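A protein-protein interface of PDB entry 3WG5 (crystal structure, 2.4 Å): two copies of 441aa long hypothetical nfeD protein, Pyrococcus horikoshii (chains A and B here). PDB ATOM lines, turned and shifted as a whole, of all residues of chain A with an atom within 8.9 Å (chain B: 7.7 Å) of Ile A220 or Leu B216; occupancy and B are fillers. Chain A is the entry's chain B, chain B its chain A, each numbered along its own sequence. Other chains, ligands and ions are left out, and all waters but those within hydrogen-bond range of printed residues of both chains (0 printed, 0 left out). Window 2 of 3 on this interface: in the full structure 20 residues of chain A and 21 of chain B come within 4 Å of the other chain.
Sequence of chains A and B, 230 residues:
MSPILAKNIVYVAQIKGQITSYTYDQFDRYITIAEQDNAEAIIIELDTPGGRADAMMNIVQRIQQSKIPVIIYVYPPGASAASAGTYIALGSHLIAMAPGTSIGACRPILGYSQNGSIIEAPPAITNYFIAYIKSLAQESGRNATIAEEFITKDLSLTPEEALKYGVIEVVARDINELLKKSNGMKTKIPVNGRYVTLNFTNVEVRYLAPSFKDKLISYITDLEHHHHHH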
ATOM      1  N   TYR A  22     -26.974 -23.862 -24.330  1.00  0.00           N
ATOM      2  CA  TYR A  22     -28.183 -24.575 -23.923  1.00  0.00           C
ATOM      3  C   TYR A  22     -29.340 -24.155 -24.817  1.00  0.00           C
ATOM      4  O   TYR A  22     -30.229 -24.963 -25.112  1.00  0.00           O
ATOM      5  CB  TYR A  22     -28.538 -24.317 -22.450  1.00  0.00           C
ATOM      6  CG  TYR A  22     -27.423 -24.575 -21.457  1.00  0.00           C
ATOM      7  CD1 TYR A  22     -26.746 -23.514 -20.859  1.00  0.00           C
ATOM      8  CD2 TYR A  22     -27.062 -25.880 -21.096  1.00  0.00           C
ATOM      9  CE1 TYR A  22     -25.727 -23.740 -19.930  1.00  0.00           C
ATOM     10  CE2 TYR A  22     -26.043 -26.117 -20.170  1.00  0.00           C
ATOM     11  CZ  TYR A  22     -25.382 -25.042 -19.596  1.00  0.00           C
ATOM     12  OH  TYR A  22     -24.376 -25.258 -18.683  1.00  0.00           O
ATOM     13  N   LYS A 213     -33.881 -30.522 -18.039  1.00  0.00           N
ATOM     14  CA  LYS A 213     -32.642 -29.766 -18.169  1.00  0.00           C
ATOM     15  C   LYS A 213     -32.926 -28.287 -18.478  1.00  0.00           C
ATOM     16  O   LYS A 213     -32.332 -27.402 -17.855  1.00  0.00           O
ATOM     17  CB  LYS A 213     -31.749 -30.395 -19.241  1.00  0.00           C
ATOM     18  CG  LYS A 213     -30.437 -29.653 -19.524  1.00  0.00           C
ATOM     19  CD  LYS A 213     -29.631 -30.352 -20.619  1.00  0.00           C
ATOM     20  CE  LYS A 213     -28.187 -29.879 -20.622  1.00  0.00           C
ATOM     21  NZ  LYS A 213     -27.361 -30.681 -21.560  1.00  0.00           N
ATOM     22  N   ASP A 214     -33.853 -28.032 -19.404  1.00  0.00           N
ATOM     23  CA  ASP A 214     -34.271 -26.668 -19.733  1.00  0.00           C
ATOM     24  C   ASP A 214     -34.715 -25.910 -18.490  1.00  0.00           C
ATOM     25  O   ASP A 214     -34.249 -24.807 -18.229  1.00  0.00           O
ATOM     26  CB  ASP A 214     -35.430 -26.660 -20.742  1.00  0.00           C
ATOM     27  CG  ASP A 214     -35.031 -27.156 -22.120  1.00  0.00           C
ATOM     28  OD1 ASP A 214     -35.933 -27.571 -22.895  1.00  0.00           O
ATOM     29  OD2 ASP A 214     -33.824 -27.113 -22.436  1.00  0.00           O
ATOM     30  N   LYS A 215     -35.631 -26.516 -17.739  1.00  0.00           N
ATOM     31  CA  LYS A 215     -36.228 -25.901 -16.562  1.00  0.00           C
ATOM     32  C   LYS A 215     -35.207 -25.633 -15.456  1.00  0.00           C
ATOM     33  O   LYS A 215     -35.211 -24.554 -14.853  1.00  0.00           O
ATOM     34  CB  LYS A 215     -37.386 -26.762 -16.058  1.00  0.00           C
ATOM     35  CG  LYS A 215     -38.547 -26.837 -17.043  1.00  0.00           C
ATOM     36  CD  LYS A 215     -39.404 -28.072 -16.826  1.00  0.00           C
ATOM     37  CE  LYS A 215     -40.733 -27.739 -16.165  1.00  0.00           C
ATOM     38  NZ  LYS A 215     -41.614 -26.931 -17.058  1.00  0.00           N
ATOM     39  N   LEU A 216     -34.323 -26.601 -15.211  1.00  0.00           N
ATOM     40  CA  LEU A 216     -33.287 -26.459 -14.196  1.00  0.00           C
ATOM     41  C   LEU A 216     -32.362 -25.282 -14.491  1.00  0.00           C
ATOM     42  O   LEU A 216     -32.148 -24.424 -13.623  1.00  0.00           O
ATOM     43  CB  LEU A 216     -32.468 -27.743 -14.040  1.00  0.00           C
ATOM     44  CG  LEU A 216     -31.409 -27.639 -12.937  1.00  0.00           C
ATOM     45  CD1 LEU A 216     -31.993 -28.018 -11.585  1.00  0.00           C
ATOM     46  CD2 LEU A 216     -30.173 -28.467 -13.246  1.00  0.00           C
ATOM     47  N   ILE A 217     -31.816 -25.246 -15.707  1.00  0.00           N
ATOM     48  CA  ILE A 217     -30.881 -24.187 -16.110  1.00  0.00           C
ATOM     49  C   ILE A 217     -31.524 -22.804 -15.940  1.00  0.00           C
ATOM     50  O   ILE A 217     -30.884 -21.872 -15.441  1.00  0.00           O
ATOM     51  CB  ILE A 217     -30.363 -24.398 -17.571  1.00  0.00           C
ATOM     52  CG1 ILE A 217     -29.567 -25.707 -17.702  1.00  0.00           C
ATOM     53  CG2 ILE A 217     -29.547 -23.204 -18.069  1.00  0.00           C
ATOM     54  CD1 ILE A 217     -28.507 -25.936 -16.633  1.00  0.00           C
ATOM     55  N   SER A 218     -32.795 -22.690 -16.320  1.00  0.00           N
ATOM     56  CA  SER A 218     -33.498 -21.411 -16.243  1.00  0.00           C
ATOM     57  C   SER A 218     -33.905 -21.011 -14.816  1.00  0.00           C
ATOM     58  O   SER A 218     -33.923 -19.821 -14.488  1.00  0.00           O
ATOM     59  CB  SER A 218     -34.690 -21.366 -17.205  1.00  0.00           C
ATOM     60  OG  SER A 218     -35.821 -22.024 -16.673  1.00  0.00           O
ATOM     61  N   TYR A 219     -34.223 -21.991 -13.969  1.00  0.00           N
ATOM     62  CA  TYR A 219     -34.487 -21.693 -12.567  1.00  0.00           C
ATOM     63  C   TYR A 219     -33.234 -21.186 -11.865  1.00  0.00           C
ATOM     64  O   TYR A 219     -33.317 -20.253 -11.072  1.00  0.00           O
ATOM     65  CB  TYR A 219     -35.079 -22.884 -11.822  1.00  0.00           C
ATOM     66  CG  TYR A 219     -35.409 -22.576 -10.374  1.00  0.00           C
ATOM     67  CD1 TYR A 219     -36.608 -21.953 -10.031  1.00  0.00           C
ATOM     68  CD2 TYR A 219     -34.517 -22.887  -9.355  1.00  0.00           C
ATOM     69  CE1 TYR A 219     -36.920 -21.662  -8.702  1.00  0.00           C
ATOM     70  CE2 TYR A 219     -34.818 -22.599  -8.021  1.00  0.00           C
ATOM     71  CZ  TYR A 219     -36.022 -21.989  -7.704  1.00  0.00           C
ATOM     72  OH  TYR A 219     -36.332 -21.703  -6.387  1.00  0.00           O
ATOM     73  N   ILE A 220     -32.081 -21.792 -12.155  1.00  0.00           N
ATOM     74  CA  ILE A 220     -30.801 -21.296 -11.646  1.00  0.00           C
ATOM     75  C   ILE A 220     -30.573 -19.856 -12.099  1.00  0.00           C
ATOM     76  O   ILE A 220     -30.117 -19.012 -11.324  1.00  0.00           O
ATOM     77  CB  ILE A 220     -29.617 -22.168 -12.105  1.00  0.00           C
ATOM     78  CG1 ILE A 220     -29.700 -23.547 -11.453  1.00  0.00           C
ATOM     79  CG2 ILE A 220     -28.271 -21.490 -11.776  1.00  0.00           C
ATOM     80  CD1 ILE A 220     -28.627 -24.499 -11.901  1.00  0.00           C
ATOM     81  N   THR A 221     -30.902 -19.595 -13.362  1.00  0.00           N
ATOM     82  CA  THR A 221     -30.802 -18.271 -13.974  1.00  0.00           C
ATOM     83  C   THR A 221     -31.684 -17.226 -13.271  1.00  0.00           C
ATOM     84  O   THR A 221     -31.226 -16.115 -12.993  1.00  0.00           O
ATOM     85  CB  THR A 221     -31.092 -18.356 -15.503  1.00  0.00           C
ATOM     86  OG1 THR A 221     -29.885 -18.720 -16.191  1.00  0.00           O
ATOM     87  CG2 THR A 221     -31.631 -17.034 -16.063  1.00  0.00           C
ATOM     88  N   ASP A 222     -32.925 -17.600 -12.964  1.00  0.00           N
ATOM     89  CA  ASP A 222     -33.861 -16.732 -12.226  1.00  0.00           C
ATOM     90  C   ASP A 222     -33.398 -16.334 -10.797  1.00  0.00           C
ATOM     91  O   ASP A 222     -34.150 -15.688 -10.058  1.00  0.00           O
ATOM     92  CB  ASP A 222     -35.255 -17.383 -12.163  1.00  0.00           C
ATOM     93  CG  ASP A 222     -35.946 -17.462 -13.523  1.00  0.00           C
ATOM     94  OD1 ASP A 222     -35.400 -16.955 -14.533  1.00  0.00           O
ATOM     95  OD2 ASP A 222     -37.055 -18.038 -13.577  1.00  0.00           O
ATOM     96  N   LEU A 223     -32.175 -16.719 -10.424  1.00  0.00           N
ATOM     97  CA  LEU A 223     -31.596 -16.378  -9.117  1.00  0.00           C
ATOM     98  C   LEU A 223     -30.253 -15.654  -9.270  1.00  0.00           C
ATOM     99  O   LEU A 223     -29.847 -15.277 -10.376  1.00  0.00           O
ATOM    100  CB  LEU A 223     -31.418 -17.635  -8.239  1.00  0.00           C
ATOM    101  CG  LEU A 223     -32.530 -18.697  -8.104  1.00  0.00           C
ATOM    102  CD1 LEU A 223     -32.047 -19.912  -7.311  1.00  0.00           C
ATOM    103  CD2 LEU A 223     -33.829 -18.151  -7.495  1.00  0.00           C
ATOM    104  N   TYR B  22     -20.067 -16.120 -13.764  1.00  0.00           N
ATOM    105  CA  TYR B  22     -20.106 -16.670 -12.420  1.00  0.00           C
ATOM    106  C   TYR B  22     -18.699 -16.816 -11.783  1.00  0.00           C
ATOM    107  O   TYR B  22     -18.552 -16.724 -10.556  1.00  0.00           O
ATOM    108  CB  TYR B  22     -20.935 -17.969 -12.342  1.00  0.00           C
ATOM    109  CG  TYR B  22     -21.129 -18.394 -10.903  1.00  0.00           C
ATOM    110  CD1 TYR B  22     -21.963 -17.665 -10.036  1.00  0.00           C
ATOM    111  CD2 TYR B  22     -20.422 -19.478 -10.377  1.00  0.00           C
ATOM    112  CE1 TYR B  22     -22.110 -18.033  -8.693  1.00  0.00           C
ATOM    113  CE2 TYR B  22     -20.565 -19.854  -9.037  1.00  0.00           C
ATOM    114  CZ  TYR B  22     -21.404 -19.131  -8.208  1.00  0.00           C
ATOM    115  OH  TYR B  22     -21.525 -19.521  -6.896  1.00  0.00           O
ATOM    116  N   SER B 211     -18.667 -23.024  -2.376  1.00  0.00           N
ATOM    117  CA  SER B 211     -20.029 -23.242  -1.922  1.00  0.00           C
ATOM    118  C   SER B 211     -20.727 -24.324  -2.756  1.00  0.00           C
ATOM    119  O   SER B 211     -20.218 -24.767  -3.803  1.00  0.00           O
ATOM    120  CB  SER B 211     -20.818 -21.939  -2.017  1.00  0.00           C
ATOM    121  OG  SER B 211     -21.128 -21.647  -3.363  1.00  0.00           O
ATOM    122  N   PHE B 212     -21.907 -24.727  -2.300  1.00  0.00           N
ATOM    123  CA  PHE B 212     -22.715 -25.666  -3.055  1.00  0.00           C
ATOM    124  C   PHE B 212     -22.980 -25.113  -4.439  1.00  0.00           C
ATOM    125  O   PHE B 212     -22.865 -25.837  -5.426  1.00  0.00           O
ATOM    126  CB  PHE B 212     -24.034 -25.977  -2.342  1.00  0.00           C
ATOM    127  CG  PHE B 212     -24.982 -26.800  -3.170  1.00  0.00           C
ATOM    128  CD1 PHE B 212     -24.932 -28.183  -3.129  1.00  0.00           C
ATOM    129  CD2 PHE B 212     -25.918 -26.186  -3.988  1.00  0.00           C
ATOM    130  CE1 PHE B 212     -25.803 -28.945  -3.895  1.00  0.00           C
ATOM    131  CE2 PHE B 212     -26.796 -26.935  -4.746  1.00  0.00           C
ATOM    132  CZ  PHE B 212     -26.740 -28.318  -4.700  1.00  0.00           C
ATOM    133  N   LYS B 213     -23.333 -23.831  -4.508  1.00  0.00           N
ATOM    134  CA  LYS B 213     -23.602 -23.180  -5.791  1.00  0.00           C
ATOM    135  C   LYS B 213     -22.378 -23.198  -6.715  1.00  0.00           C
ATOM    136  O   LYS B 213     -22.525 -23.464  -7.907  1.00  0.00           O
ATOM    137  CB  LYS B 213     -24.138 -21.754  -5.604  1.00  0.00           C
ATOM    138  CG  LYS B 213     -24.721 -21.128  -6.880  1.00  0.00           C
ATOM    139  CD  LYS B 213     -24.936 -19.617  -6.735  1.00  0.00           C
ATOM    140  CE  LYS B 213     -25.600 -19.030  -7.985  1.00  0.00           C
ATOM    141  NZ  LYS B 213     -25.536 -17.531  -8.026  1.00  0.00           N
ATOM    142  N   ASP B 214     -21.184 -22.944  -6.161  1.00  0.00           N
ATOM    143  CA  ASP B 214     -19.934 -23.002  -6.949  1.00  0.00           C
ATOM    144  C   ASP B 214     -19.752 -24.382  -7.572  1.00  0.00           C
ATOM    145  O   ASP B 214     -19.639 -24.501  -8.784  1.00  0.00           O
ATOM    146  CB  ASP B 214     -18.684 -22.676  -6.106  1.00  0.00           C
ATOM    147  CG  ASP B 214     -18.718 -21.283  -5.489  1.00  0.00           C
ATOM    148  OD1 ASP B 214     -18.140 -21.140  -4.395  1.00  0.00           O
ATOM    149  OD2 ASP B 214     -19.308 -20.349  -6.071  1.00  0.00           O
ATOM    150  N   LYS B 215     -19.726 -25.420  -6.740  1.00  0.00           N
ATOM    151  CA  LYS B 215     -19.546 -26.779  -7.231  1.00  0.00           C
ATOM    152  C   LYS B 215     -20.626 -27.185  -8.236  1.00  0.00           C
ATOM    153  O   LYS B 215     -20.310 -27.744  -9.291  1.00  0.00           O
ATOM    154  CB  LYS B 215     -19.429 -27.769  -6.066  1.00  0.00           C
ATOM    155  CG  LYS B 215     -18.017 -27.801  -5.470  1.00  0.00           C
ATOM    156  CD  LYS B 215     -18.021 -27.761  -3.942  1.00  0.00           C
ATOM    157  CE  LYS B 215     -17.852 -29.140  -3.307  1.00  0.00           C
ATOM    158  NZ  LYS B 215     -18.105 -29.109  -1.831  1.00  0.00           N
ATOM    159  N   LEU B 216     -21.885 -26.868  -7.948  1.00  0.00           N
ATOM    160  CA  LEU B 216     -22.974 -27.267  -8.839  1.00  0.00           C
ATOM    161  C   LEU B 216     -22.868 -26.613 -10.213  1.00  0.00           C
ATOM    162  O   LEU B 216     -22.951 -27.297 -11.238  1.00  0.00           O
ATOM    163  CB  LEU B 216     -24.346 -26.960  -8.240  1.00  0.00           C
ATOM    164  CG  LEU B 216     -25.482 -27.376  -9.176  1.00  0.00           C
ATOM    165  CD1 LEU B 216     -26.004 -28.758  -8.779  1.00  0.00           C
ATOM    166  CD2 LEU B 216     -26.595 -26.333  -9.225  1.00  0.00           C
ATOM    167  N   ILE B 217     -22.706 -25.287 -10.221  1.00  0.00           N
ATOM    168  CA  ILE B 217     -22.654 -24.520 -11.470  1.00  0.00           C
ATOM    169  C   ILE B 217     -21.433 -24.907 -12.300  1.00  0.00           C
ATOM    170  O   ILE B 217     -21.533 -25.032 -13.516  1.00  0.00           O
ATOM    171  CB  ILE B 217     -22.794 -22.985 -11.237  1.00  0.00           C
ATOM    172  CG1 ILE B 217     -24.270 -22.649 -10.973  1.00  0.00           C
ATOM    173  CG2 ILE B 217     -22.265 -22.176 -12.432  1.00  0.00           C
ATOM    174  CD1 ILE B 217     -24.570 -21.171 -10.727  1.00  0.00           C
ATOM    175  N   SER B 218     -20.304 -25.137 -11.633  1.00  0.00           N
ATOM    176  CA  SER B 218     -19.103 -25.649 -12.292  1.00  0.00           C
ATOM    177  C   SER B 218     -19.395 -26.991 -12.954  1.00  0.00           C
ATOM    178  O   SER B 218     -19.114 -27.163 -14.138  1.00  0.00           O
ATOM    179  CB  SER B 218     -17.927 -25.786 -11.309  1.00  0.00           C
ATOM    180  OG  SER B 218     -17.302 -24.534 -11.061  1.00  0.00           O
ATOM    181  N   TYR B 219     -19.967 -27.923 -12.190  1.00  0.00           N
ATOM    182  CA  TYR B 219     -20.300 -29.260 -12.692  1.00  0.00           C
ATOM    183  C   TYR B 219     -21.229 -29.222 -13.897  1.00  0.00           C
ATOM    184  O   TYR B 219     -21.097 -30.045 -14.800  1.00  0.00           O
ATOM    185  CB  TYR B 219     -20.906 -30.136 -11.588  1.00  0.00           C
ATOM    186  CG  TYR B 219     -21.222 -31.558 -12.016  1.00  0.00           C
ATOM    187  CD1 TYR B 219     -20.248 -32.555 -11.967  1.00  0.00           C
ATOM    188  CD2 TYR B 219     -22.494 -31.907 -12.474  1.00  0.00           C
ATOM    189  CE1 TYR B 219     -20.535 -33.870 -12.357  1.00  0.00           C
ATOM    190  CE2 TYR B 219     -22.789 -33.212 -12.873  1.00  0.00           C
ATOM    191  CZ  TYR B 219     -21.807 -34.187 -12.812  1.00  0.00           C
ATOM    192  OH  TYR B 219     -22.093 -35.477 -13.202  1.00  0.00           O
ATOM    193  N   ILE B 220     -22.166 -28.277 -13.907  1.00  0.00           N
ATOM    194  CA  ILE B 220     -23.139 -28.172 -14.995  1.00  0.00           C
ATOM    195  C   ILE B 220     -22.503 -27.625 -16.277  1.00  0.00           C
ATOM    196  O   ILE B 220     -22.760 -28.133 -17.372  1.00  0.00           O
ATOM    197  CB  ILE B 220     -24.362 -27.329 -14.583  1.00  0.00           C
ATOM    198  CG1 ILE B 220     -25.263 -28.131 -13.644  1.00  0.00           C
ATOM    199  CG2 ILE B 220     -25.155 -26.883 -15.802  1.00  0.00           C
ATOM    200  CD1 ILE B 220     -26.382 -27.318 -13.045  1.00  0.00           C
ATOM    201  N   THR B 221     -21.679 -26.588 -16.133  1.00  0.00           N
ATOM    202  CA  THR B 221     -20.913 -26.029 -17.248  1.00  0.00           C
ATOM    203  C   THR B 221     -19.952 -27.076 -17.823  1.00  0.00           C
ATOM    204  O   THR B 221     -19.678 -27.083 -19.024  1.00  0.00           O
ATOM    205  CB  THR B 221     -20.146 -24.761 -16.820  1.00  0.00           C
ATOM    206  OG1 THR B 221     -21.047 -23.870 -16.148  1.00  0.00           O
ATOM    207  CG2 THR B 221     -19.544 -24.043 -18.029  1.00  0.00           C
ATOM    208  N   ASP B 222     -19.490 -27.977 -16.961  1.00  0.00           N
ATOM    209  CA  ASP B 222     -18.621 -29.082 -17.352  1.00  0.00           C
ATOM    210  C   ASP B 222     -19.200 -29.953 -18.466  1.00  0.00           C
ATOM    211  O   ASP B 222     -18.471 -30.360 -19.370  1.00  0.00           O
ATOM    212  CB  ASP B 222     -18.316 -29.954 -16.135  1.00  0.00           C
ATOM    213  CG  ASP B 222     -16.831 -30.107 -15.882  1.00  0.00           C
ATOM    214  OD1 ASP B 222     -16.078 -29.126 -16.085  1.00  0.00           O
ATOM    215  OD2 ASP B 222     -16.420 -31.209 -15.461  1.00  0.00           O
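The backbone carbonyl oxygen of Ile B217 lies within hydrogen-bond range of the side-chain hydroxyl of Thr B221.
The backbone carbonyl oxygen of Ile A217 lies within hydrogen-bond range of the side-chain hydroxyl of Thr A221 (3.4 Å).
Among the printed residues, merely in contact across the chains: Tyr A22 with Ile B220, Tyr A22 with Thr B221, Leu A216 with Ile B220, Ile A217 with Ile B220, Ile A220 with Leu B216, Ile A220 with Ile B217 and Ile A220 with Ile B220.
Of the printed residues of chain B, Tyr A22 touches Ile B220 and Thr B221.
Printed residues of chain B within 4 Å of Leu A216: Ile B220.
Printed residues of chain B within 4 Å of Ile A217: Ile B220 (3.6 Å).
Ile A220 touches three residues of chain B.
Leu B216 touches just one residue of chain A: Ile A220 (3.8 Å).
Of the printed residues of chain A, Ile B217 touches Ile A220.
Of the printed residues of chain A, Thr B221 touches Tyr A22 (3.8 Å).
The nearest residue of chain B that does not touch Ile A220 is Lys B213 (5.2 Å).
Printed residues of chain A that touch a printed residue of chain B: Tyr A22, Leu A216, Ile A217 and Ile A220.
Printed residues of chain B that touch a printed residue of chain A: Leu B216, Ile B217, Ile B220 and Thr B221.
Among the printed residues, no Asp or Glu carboxylate lies within 4 Å of a Lys or Arg side-chain nitrogen of the other chain.
Tyr A22 touches Ile B220, but with the chains exchanged Ile A220 does not touch Tyr B22 (7.6 Å).
Tyr A22 touches Thr B221, but with the chains exchanged Thr A221 does not touch Tyr B22 (9.7 Å).
Leu A216 touches Ile B220, and with the chains exchanged Ile A220 touches Leu B216.
Ile A217 touches Ile B220, and with the chains exchanged Ile A220 touches Ile B217.
Of the 7 pairs that touch across the chains among the printed residues, 5 have their exchanged pair printed and touching as well.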
